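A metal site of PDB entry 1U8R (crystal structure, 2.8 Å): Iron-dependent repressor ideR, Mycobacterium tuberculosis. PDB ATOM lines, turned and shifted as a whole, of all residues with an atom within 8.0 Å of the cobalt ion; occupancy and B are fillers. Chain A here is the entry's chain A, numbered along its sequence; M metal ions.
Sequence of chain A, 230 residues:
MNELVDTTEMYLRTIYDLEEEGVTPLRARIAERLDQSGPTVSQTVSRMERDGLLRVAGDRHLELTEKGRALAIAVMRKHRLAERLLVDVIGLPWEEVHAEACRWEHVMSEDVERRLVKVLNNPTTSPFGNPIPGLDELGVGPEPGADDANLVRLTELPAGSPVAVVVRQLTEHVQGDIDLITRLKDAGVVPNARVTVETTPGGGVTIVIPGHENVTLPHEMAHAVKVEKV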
ATOM      1  N   ARG A  13       7.692 -13.732  18.393  1.00  0.00           N
ATOM      2  CA  ARG A  13       6.960 -14.761  19.129  1.00  0.00           C
ATOM      3  C   ARG A  13       5.929 -15.465  18.246  1.00  0.00           C
ATOM      4  O   ARG A  13       5.677 -16.663  18.425  1.00  0.00           O
ATOM      5  CB  ARG A  13       6.282 -14.162  20.369  1.00  0.00           C
ATOM      6  CG  ARG A  13       6.321 -15.089  21.568  1.00  0.00           C
ATOM      7  CD  ARG A  13       4.960 -15.662  21.864  1.00  0.00           C
ATOM      8  NE  ARG A  13       4.092 -14.678  22.470  1.00  0.00           N
ATOM      9  CZ  ARG A  13       2.774 -14.618  22.350  1.00  0.00           C
ATOM     10  NH1 ARG A  13       2.108 -15.496  21.616  1.00  0.00           N
ATOM     11  NH2 ARG A  13       2.114 -13.656  22.992  1.00  0.00           N
ATOM     12  N   ASP A  17       5.682 -19.291  17.732  1.00  0.00           N
ATOM     13  CA  ASP A  17       4.407 -19.973  17.916  1.00  0.00           C
ATOM     14  C   ASP A  17       4.070 -20.884  16.748  1.00  0.00           C
ATOM     15  O   ASP A  17       3.683 -22.027  16.941  1.00  0.00           O
ATOM     16  CB  ASP A  17       3.274 -18.978  18.097  1.00  0.00           C
ATOM     17  CG  ASP A  17       3.149 -18.500  19.517  1.00  0.00           C
ATOM     18  OD1 ASP A  17       3.076 -19.371  20.421  1.00  0.00           O
ATOM     19  OD2 ASP A  17       3.114 -17.276  19.737  1.00  0.00           O
ATOM     20  N   MET A  76       8.972 -15.623  24.919  1.00  0.00           N
ATOM     21  CA  MET A  76       8.138 -16.769  25.247  1.00  0.00           C
ATOM     22  C   MET A  76       8.293 -17.170  26.712  1.00  0.00           C
ATOM     23  O   MET A  76       7.313 -17.541  27.353  1.00  0.00           O
ATOM     24  CB  MET A  76       8.505 -17.958  24.354  1.00  0.00           C
ATOM     25  CG  MET A  76       7.605 -19.127  24.580  1.00  0.00           C
ATOM     26  SD  MET A  76       5.887 -18.666  24.350  1.00  0.00           S
ATOM     27  CE  MET A  76       5.639 -19.153  22.646  1.00  0.00           C
ATOM     28  N   HIS A  79       6.628 -14.729  29.055  1.00  0.00           N
ATOM     29  CA  HIS A  79       5.217 -14.974  28.863  1.00  0.00           C
ATOM     30  C   HIS A  79       4.745 -16.085  29.770  1.00  0.00           C
ATOM     31  O   HIS A  79       3.879 -15.876  30.606  1.00  0.00           O
ATOM     32  CB  HIS A  79       4.923 -15.357  27.407  1.00  0.00           C
ATOM     33  CG  HIS A  79       3.490 -15.729  27.177  1.00  0.00           C
ATOM     34  ND1 HIS A  79       2.465 -14.804  27.162  1.00  0.00           N
ATOM     35  CD2 HIS A  79       2.902 -16.933  26.986  1.00  0.00           C
ATOM     36  CE1 HIS A  79       1.309 -15.429  26.974  1.00  0.00           C
ATOM     37  NE2 HIS A  79       1.548 -16.717  26.868  1.00  0.00           N
ATOM     38  N   ARG A  80       5.341 -17.266  29.632  1.00  0.00           N
ATOM     39  CA  ARG A  80       4.925 -18.395  30.456  1.00  0.00           C
ATOM     40  C   ARG A  80       5.196 -18.272  31.944  1.00  0.00           C
ATOM     41  O   ARG A  80       4.382 -18.706  32.747  1.00  0.00           O
ATOM     42  CB  ARG A  80       5.516 -19.673  29.865  1.00  0.00           C
ATOM     43  CG  ARG A  80       4.836 -19.951  28.543  1.00  0.00           C
ATOM     44  CD  ARG A  80       5.477 -20.964  27.618  1.00  0.00           C
ATOM     45  NE  ARG A  80       4.706 -20.964  26.368  1.00  0.00           N
ATOM     46  CZ  ARG A  80       4.883 -21.797  25.353  1.00  0.00           C
ATOM     47  NH1 ARG A  80       5.800 -22.736  25.403  1.00  0.00           N
ATOM     48  NH2 ARG A  80       4.120 -21.678  24.267  1.00  0.00           N
ATOM     49  N   GLU A  83       2.238 -16.283  33.169  1.00  0.00           N
ATOM     50  CA  GLU A  83       0.990 -17.014  33.225  1.00  0.00           C
ATOM     51  C   GLU A  83       1.054 -17.823  34.513  1.00  0.00           C
ATOM     52  O   GLU A  83       0.049 -17.996  35.202  1.00  0.00           O
ATOM     53  CB  GLU A  83       0.833 -17.936  31.994  1.00  0.00           C
ATOM     54  CG  GLU A  83       0.730 -17.174  30.673  1.00  0.00           C
ATOM     55  CD  GLU A  83       0.516 -18.068  29.450  1.00  0.00           C
ATOM     56  OE1 GLU A  83       1.271 -19.039  29.228  1.00  0.00           O
ATOM     57  OE2 GLU A  83      -0.430 -17.768  28.676  1.00  0.00           O
ATOM     58  N   VAL A  97      -5.430 -15.322  32.022  1.00  0.00           N
ATOM     59  CA  VAL A  97      -4.000 -15.094  32.179  1.00  0.00           C
ATOM     60  C   VAL A  97      -3.250 -14.936  30.864  1.00  0.00           C
ATOM     61  O   VAL A  97      -2.323 -14.141  30.760  1.00  0.00           O
ATOM     62  CB  VAL A  97      -3.340 -16.221  32.955  1.00  0.00           C
ATOM     63  CG1 VAL A  97      -3.800 -16.207  34.397  1.00  0.00           C
ATOM     64  CG2 VAL A  97      -3.664 -17.545  32.301  1.00  0.00           C
ATOM     65  N   HIS A  98      -3.644 -15.699  29.847  1.00  0.00           N
ATOM     66  CA  HIS A  98      -2.933 -15.576  28.596  1.00  0.00           C
ATOM     67  C   HIS A  98      -2.940 -14.143  28.097  1.00  0.00           C
ATOM     68  O   HIS A  98      -1.876 -13.574  27.870  1.00  0.00           O
ATOM     69  CB  HIS A  98      -3.524 -16.485  27.534  1.00  0.00           C
ATOM     70  CG  HIS A  98      -2.893 -16.294  26.191  1.00  0.00           C
ATOM     71  ND1 HIS A  98      -1.545 -16.499  25.970  1.00  0.00           N
ATOM     72  CD2 HIS A  98      -3.401 -15.832  25.029  1.00  0.00           C
ATOM     73  CE1 HIS A  98      -1.252 -16.165  24.725  1.00  0.00           C
ATOM     74  NE2 HIS A  98      -2.360 -15.757  24.127  1.00  0.00           N
ATOM     75  N   ALA A  99      -4.122 -13.552  27.921  1.00  0.00           N
ATOM     76  CA  ALA A  99      -4.215 -12.185  27.415  1.00  0.00           C
ATOM     77  C   ALA A  99      -3.431 -11.156  28.246  1.00  0.00           C
ATOM     78  O   ALA A  99      -2.934 -10.145  27.722  1.00  0.00           O
ATOM     79  CB  ALA A  99      -5.662 -11.773  27.337  1.00  0.00           C
ATOM     80  N   GLU A 100      -3.342 -11.408  29.553  1.00  0.00           N
ATOM     81  CA  GLU A 100      -2.642 -10.534  30.473  1.00  0.00           C
ATOM     82  C   GLU A 100      -1.149 -10.691  30.247  1.00  0.00           C
ATOM     83  O   GLU A 100      -0.404  -9.720  30.180  1.00  0.00           O
ATOM     84  CB  GLU A 100      -2.986 -10.921  31.889  1.00  0.00           C
ATOM     85  CG  GLU A 100      -2.424 -10.007  32.960  1.00  0.00           C
ATOM     86  CD  GLU A 100      -3.053  -8.641  32.923  1.00  0.00           C
ATOM     87  OE1 GLU A 100      -4.240  -8.550  32.519  1.00  0.00           O
ATOM     88  OE2 GLU A 100      -2.356  -7.677  33.295  1.00  0.00           O
ATOM     89  N   ALA A 101      -0.716 -11.944  30.133  1.00  0.00           N
ATOM     90  CA  ALA A 101       0.683 -12.254  29.928  1.00  0.00           C
ATOM     91  C   ALA A 101       1.192 -11.756  28.574  1.00  0.00           C
ATOM     92  O   ALA A 101       2.360 -11.414  28.433  1.00  0.00           O
ATOM     93  CB  ALA A 101       0.906 -13.755  30.028  1.00  0.00           C
ATOM     94  N   CYS A 102       0.296 -11.719  27.588  1.00  0.00           N
ATOM     95  CA  CYS A 102       0.652 -11.276  26.247  1.00  0.00           C
ATOM     96  C   CYS A 102       1.154  -9.847  26.276  1.00  0.00           C
ATOM     97  O   CYS A 102       1.805  -9.383  25.336  1.00  0.00           O
ATOM     98  CB  CYS A 102      -0.545 -11.380  25.321  1.00  0.00           C
ATOM     99  SG  CYS A 102      -0.158 -11.868  23.654  1.00  0.00           S
ATOM    100  N   GLU A 105       4.669  -9.835  28.998  1.00  0.00           N
ATOM    101  CA  GLU A 105       5.823 -10.447  28.360  1.00  0.00           C
ATOM    102  C   GLU A 105       6.770  -9.444  27.751  1.00  0.00           C
ATOM    103  O   GLU A 105       7.935  -9.741  27.536  1.00  0.00           O
ATOM    104  CB  GLU A 105       5.361 -11.414  27.299  1.00  0.00           C
ATOM    105  CG  GLU A 105       4.894 -10.731  26.046  1.00  0.00           C
ATOM    106  CD  GLU A 105       4.232 -11.703  25.131  1.00  0.00           C
ATOM    107  OE1 GLU A 105       4.400 -12.924  25.382  1.00  0.00           O
ATOM    108  OE2 GLU A 105       3.550 -11.255  24.169  1.00  0.00           O
ATOM    109  N   SER A 126       3.745 -24.050  31.679  1.00  0.00           N
ATOM    110  CA  SER A 126       2.769 -23.000  31.892  1.00  0.00           C
ATOM    111  C   SER A 126       1.471 -23.673  32.312  1.00  0.00           C
ATOM    112  O   SER A 126       1.355 -24.881  32.212  1.00  0.00           O
ATOM    113  CB  SER A 126       2.523 -22.237  30.589  1.00  0.00           C
ATOM    114  OG  SER A 126       1.884 -23.080  29.643  1.00  0.00           O
ATOM    115  N   PRO A 127       0.490 -22.894  32.798  1.00  0.00           N
ATOM    116  CA  PRO A 127      -0.804 -23.422  33.222  1.00  0.00           C
ATOM    117  C   PRO A 127      -1.512 -24.115  32.072  1.00  0.00           C
ATOM    118  O   PRO A 127      -2.653 -24.547  32.210  1.00  0.00           O
ATOM    119  CB  PRO A 127      -1.551 -22.183  33.669  1.00  0.00           C
ATOM    120  CG  PRO A 127      -0.463 -21.371  34.262  1.00  0.00           C
ATOM    121  CD  PRO A 127       0.645 -21.497  33.239  1.00  0.00           C
ATOM    122  N   PHE A 128      -0.858 -24.197  30.924  1.00  0.00           N
ATOM    123  CA  PHE A 128      -1.444 -24.843  29.765  1.00  0.00           C
ATOM    124  C   PHE A 128      -0.561 -25.977  29.290  1.00  0.00           C
ATOM    125  O   PHE A 128      -0.830 -26.597  28.255  1.00  0.00           O
ATOM    126  CB  PHE A 128      -1.686 -23.837  28.654  1.00  0.00           C
ATOM    127  CG  PHE A 128      -2.614 -22.726  29.029  1.00  0.00           C
ATOM    128  CD1 PHE A 128      -2.194 -21.716  29.891  1.00  0.00           C
ATOM    129  CD2 PHE A 128      -3.906 -22.706  28.559  1.00  0.00           C
ATOM    130  CE1 PHE A 128      -3.061 -20.701  30.275  1.00  0.00           C
ATOM    131  CE2 PHE A 128      -4.789 -21.697  28.928  1.00  0.00           C
ATOM    132  CZ  PHE A 128      -4.357 -20.685  29.796  1.00  0.00           C
ATOM    133  N   ASN A 130       2.675 -25.919  28.203  1.00  0.00           N
ATOM    134  CA  ASN A 130       3.803 -25.692  27.328  1.00  0.00           C
ATOM    135  C   ASN A 130       5.039 -25.453  28.168  1.00  0.00           C
ATOM    136  O   ASN A 130       4.984 -24.777  29.184  1.00  0.00           O
ATOM    137  CB  ASN A 130       3.489 -24.518  26.412  1.00  0.00           C
ATOM    138  CG  ASN A 130       2.086 -24.614  25.850  1.00  0.00           C
ATOM    139  OD1 ASN A 130       1.141 -24.083  26.421  1.00  0.00           O
ATOM    140  ND2 ASN A 130       1.934 -25.330  24.732  1.00  0.00           N
ATOM    141  N   LEU A 170      -1.867 -26.954  25.272  1.00  0.00           N
ATOM    142  CA  LEU A 170      -2.752 -26.061  24.547  1.00  0.00           C
ATOM    143  C   LEU A 170      -1.880 -24.854  24.211  1.00  0.00           C
ATOM    144  O   LEU A 170      -1.772 -23.907  24.987  1.00  0.00           O
ATOM    145  CB  LEU A 170      -3.944 -25.650  25.416  1.00  0.00           C
ATOM    146  CG  LEU A 170      -4.940 -26.715  25.863  1.00  0.00           C
ATOM    147  CD1 LEU A 170      -6.170 -26.018  26.445  1.00  0.00           C
ATOM    148  CD2 LEU A 170      -5.360 -27.557  24.695  1.00  0.00           C
ATOM    149  N   THR A 171      -1.231 -24.913  23.065  1.00  0.00           N
ATOM    150  CA  THR A 171      -0.327 -23.837  22.660  1.00  0.00           C
ATOM    151  C   THR A 171      -0.975 -22.471  22.526  1.00  0.00           C
ATOM    152  O   THR A 171      -2.176 -22.348  22.334  1.00  0.00           O
ATOM    153  CB  THR A 171       0.405 -24.190  21.359  1.00  0.00           C
ATOM    154  OG1 THR A 171      -0.545 -24.612  20.377  1.00  0.00           O
ATOM    155  CG2 THR A 171       1.434 -25.268  21.615  1.00  0.00           C
ATOM    156  N   GLU A 172      -0.136 -21.455  22.636  1.00  0.00           N
ATOM    157  CA  GLU A 172      -0.572 -20.068  22.563  1.00  0.00           C
ATOM    158  C   GLU A 172      -1.609 -19.761  21.485  1.00  0.00           C
ATOM    159  O   GLU A 172      -2.474 -18.926  21.694  1.00  0.00           O
ATOM    160  CB  GLU A 172       0.656 -19.183  22.387  1.00  0.00           C
ATOM    161  CG  GLU A 172       1.780 -19.435  23.373  1.00  0.00           C
ATOM    162  CD  GLU A 172       1.342 -19.298  24.821  1.00  0.00           C
ATOM    163  OE1 GLU A 172       0.379 -18.551  25.071  1.00  0.00           O
ATOM    164  OE2 GLU A 172       1.965 -19.939  25.695  1.00  0.00           O
ATOM    165  N   HIS A 173      -1.547 -20.427  20.346  1.00  0.00           N
ATOM    166  CA  HIS A 173      -2.543 -20.115  19.331  1.00  0.00           C
ATOM    167  C   HIS A 173      -3.956 -20.293  19.864  1.00  0.00           C
ATOM    168  O   HIS A 173      -4.785 -19.404  19.710  1.00  0.00           O
ATOM    169  CB  HIS A 173      -2.372 -20.966  18.060  1.00  0.00           C
ATOM    170  CG  HIS A 173      -3.306 -20.577  16.929  1.00  0.00           C
ATOM    171  ND1 HIS A 173      -3.442 -19.277  16.492  1.00  0.00           N
ATOM    172  CD2 HIS A 173      -4.120 -21.316  16.153  1.00  0.00           C
ATOM    173  CE1 HIS A 173      -4.300 -19.238  15.490  1.00  0.00           C
ATOM    174  NE2 HIS A 173      -4.733 -20.463  15.262  1.00  0.00           N
ATOM    175  N   VAL A 174      -4.220 -21.436  20.498  1.00  0.00           N
ATOM    176  CA  VAL A 174      -5.551 -21.692  21.033  1.00  0.00           C
ATOM    177  C   VAL A 174      -5.857 -20.720  22.175  1.00  0.00           C
ATOM    178  O   VAL A 174      -6.986 -20.246  22.274  1.00  0.00           O
ATOM    179  CB  VAL A 174      -5.701 -23.166  21.529  1.00  0.00           C
ATOM    180  CG1 VAL A 174      -4.736 -23.452  22.671  1.00  0.00           C
ATOM    181  CG2 VAL A 174      -7.125 -23.413  21.957  1.00  0.00           C
ATOM    182  N   GLN A 175      -4.875 -20.429  23.018  1.00  0.00           N
ATOM    183  CA  GLN A 175      -5.084 -19.482  24.110  1.00  0.00           C
ATOM    184  C   GLN A 175      -5.597 -18.170  23.509  1.00  0.00           C
ATOM    185  O   GLN A 175      -6.284 -17.371  24.153  1.00  0.00           O
ATOM    186  CB  GLN A 175      -3.768 -19.206  24.845  1.00  0.00           C
ATOM    187  CG  GLN A 175      -3.178 -20.366  25.616  1.00  0.00           C
ATOM    188  CD  GLN A 175      -1.809 -20.033  26.213  1.00  0.00           C
ATOM    189  OE1 GLN A 175      -1.556 -18.898  26.595  1.00  0.00           O
ATOM    190  NE2 GLN A 175      -0.948 -21.013  26.314  1.00  0.00           N
ATOM    191  N   GLY A 176      -5.247 -17.949  22.235  1.00  0.00           N
ATOM    192  CA  GLY A 176      -5.652 -16.740  21.558  1.00  0.00           C
ATOM    193  C   GLY A 176      -7.147 -16.573  21.492  1.00  0.00           C
ATOM    194  O   GLY A 176      -7.687 -15.621  22.047  1.00  0.00           O
HETATM  195 CO    CO M   1      -0.140 -17.688  26.828  1.00  0.00          CO
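The cobalt ion is bound by the side-chain carboxylate of Glu 83 (1.9 Å), the side-chain amide oxygen of Gln 175 (1.9 Å), a ring nitrogen (NE2) of His 79 (1.9 Å), the side-chain carboxylate of Glu 172 (2.0 Å) and a ring nitrogen (ND1) of His 98 (2.0 Å).
The guanidinium group (NE) of Arg 80 is in salt-bridge range of the side-chain carboxylate (OE2) of Glu 172. The side-chain amide nitrogen (NE2) of Gln 175 lies within hydrogen-bond range of the backbone carbonyl oxygen (O) of Leu 170 (3.3 Å). The side-chain carboxylate (OE1) of Glu 105 lies close to a ring nitrogen (ND1) of His 79.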
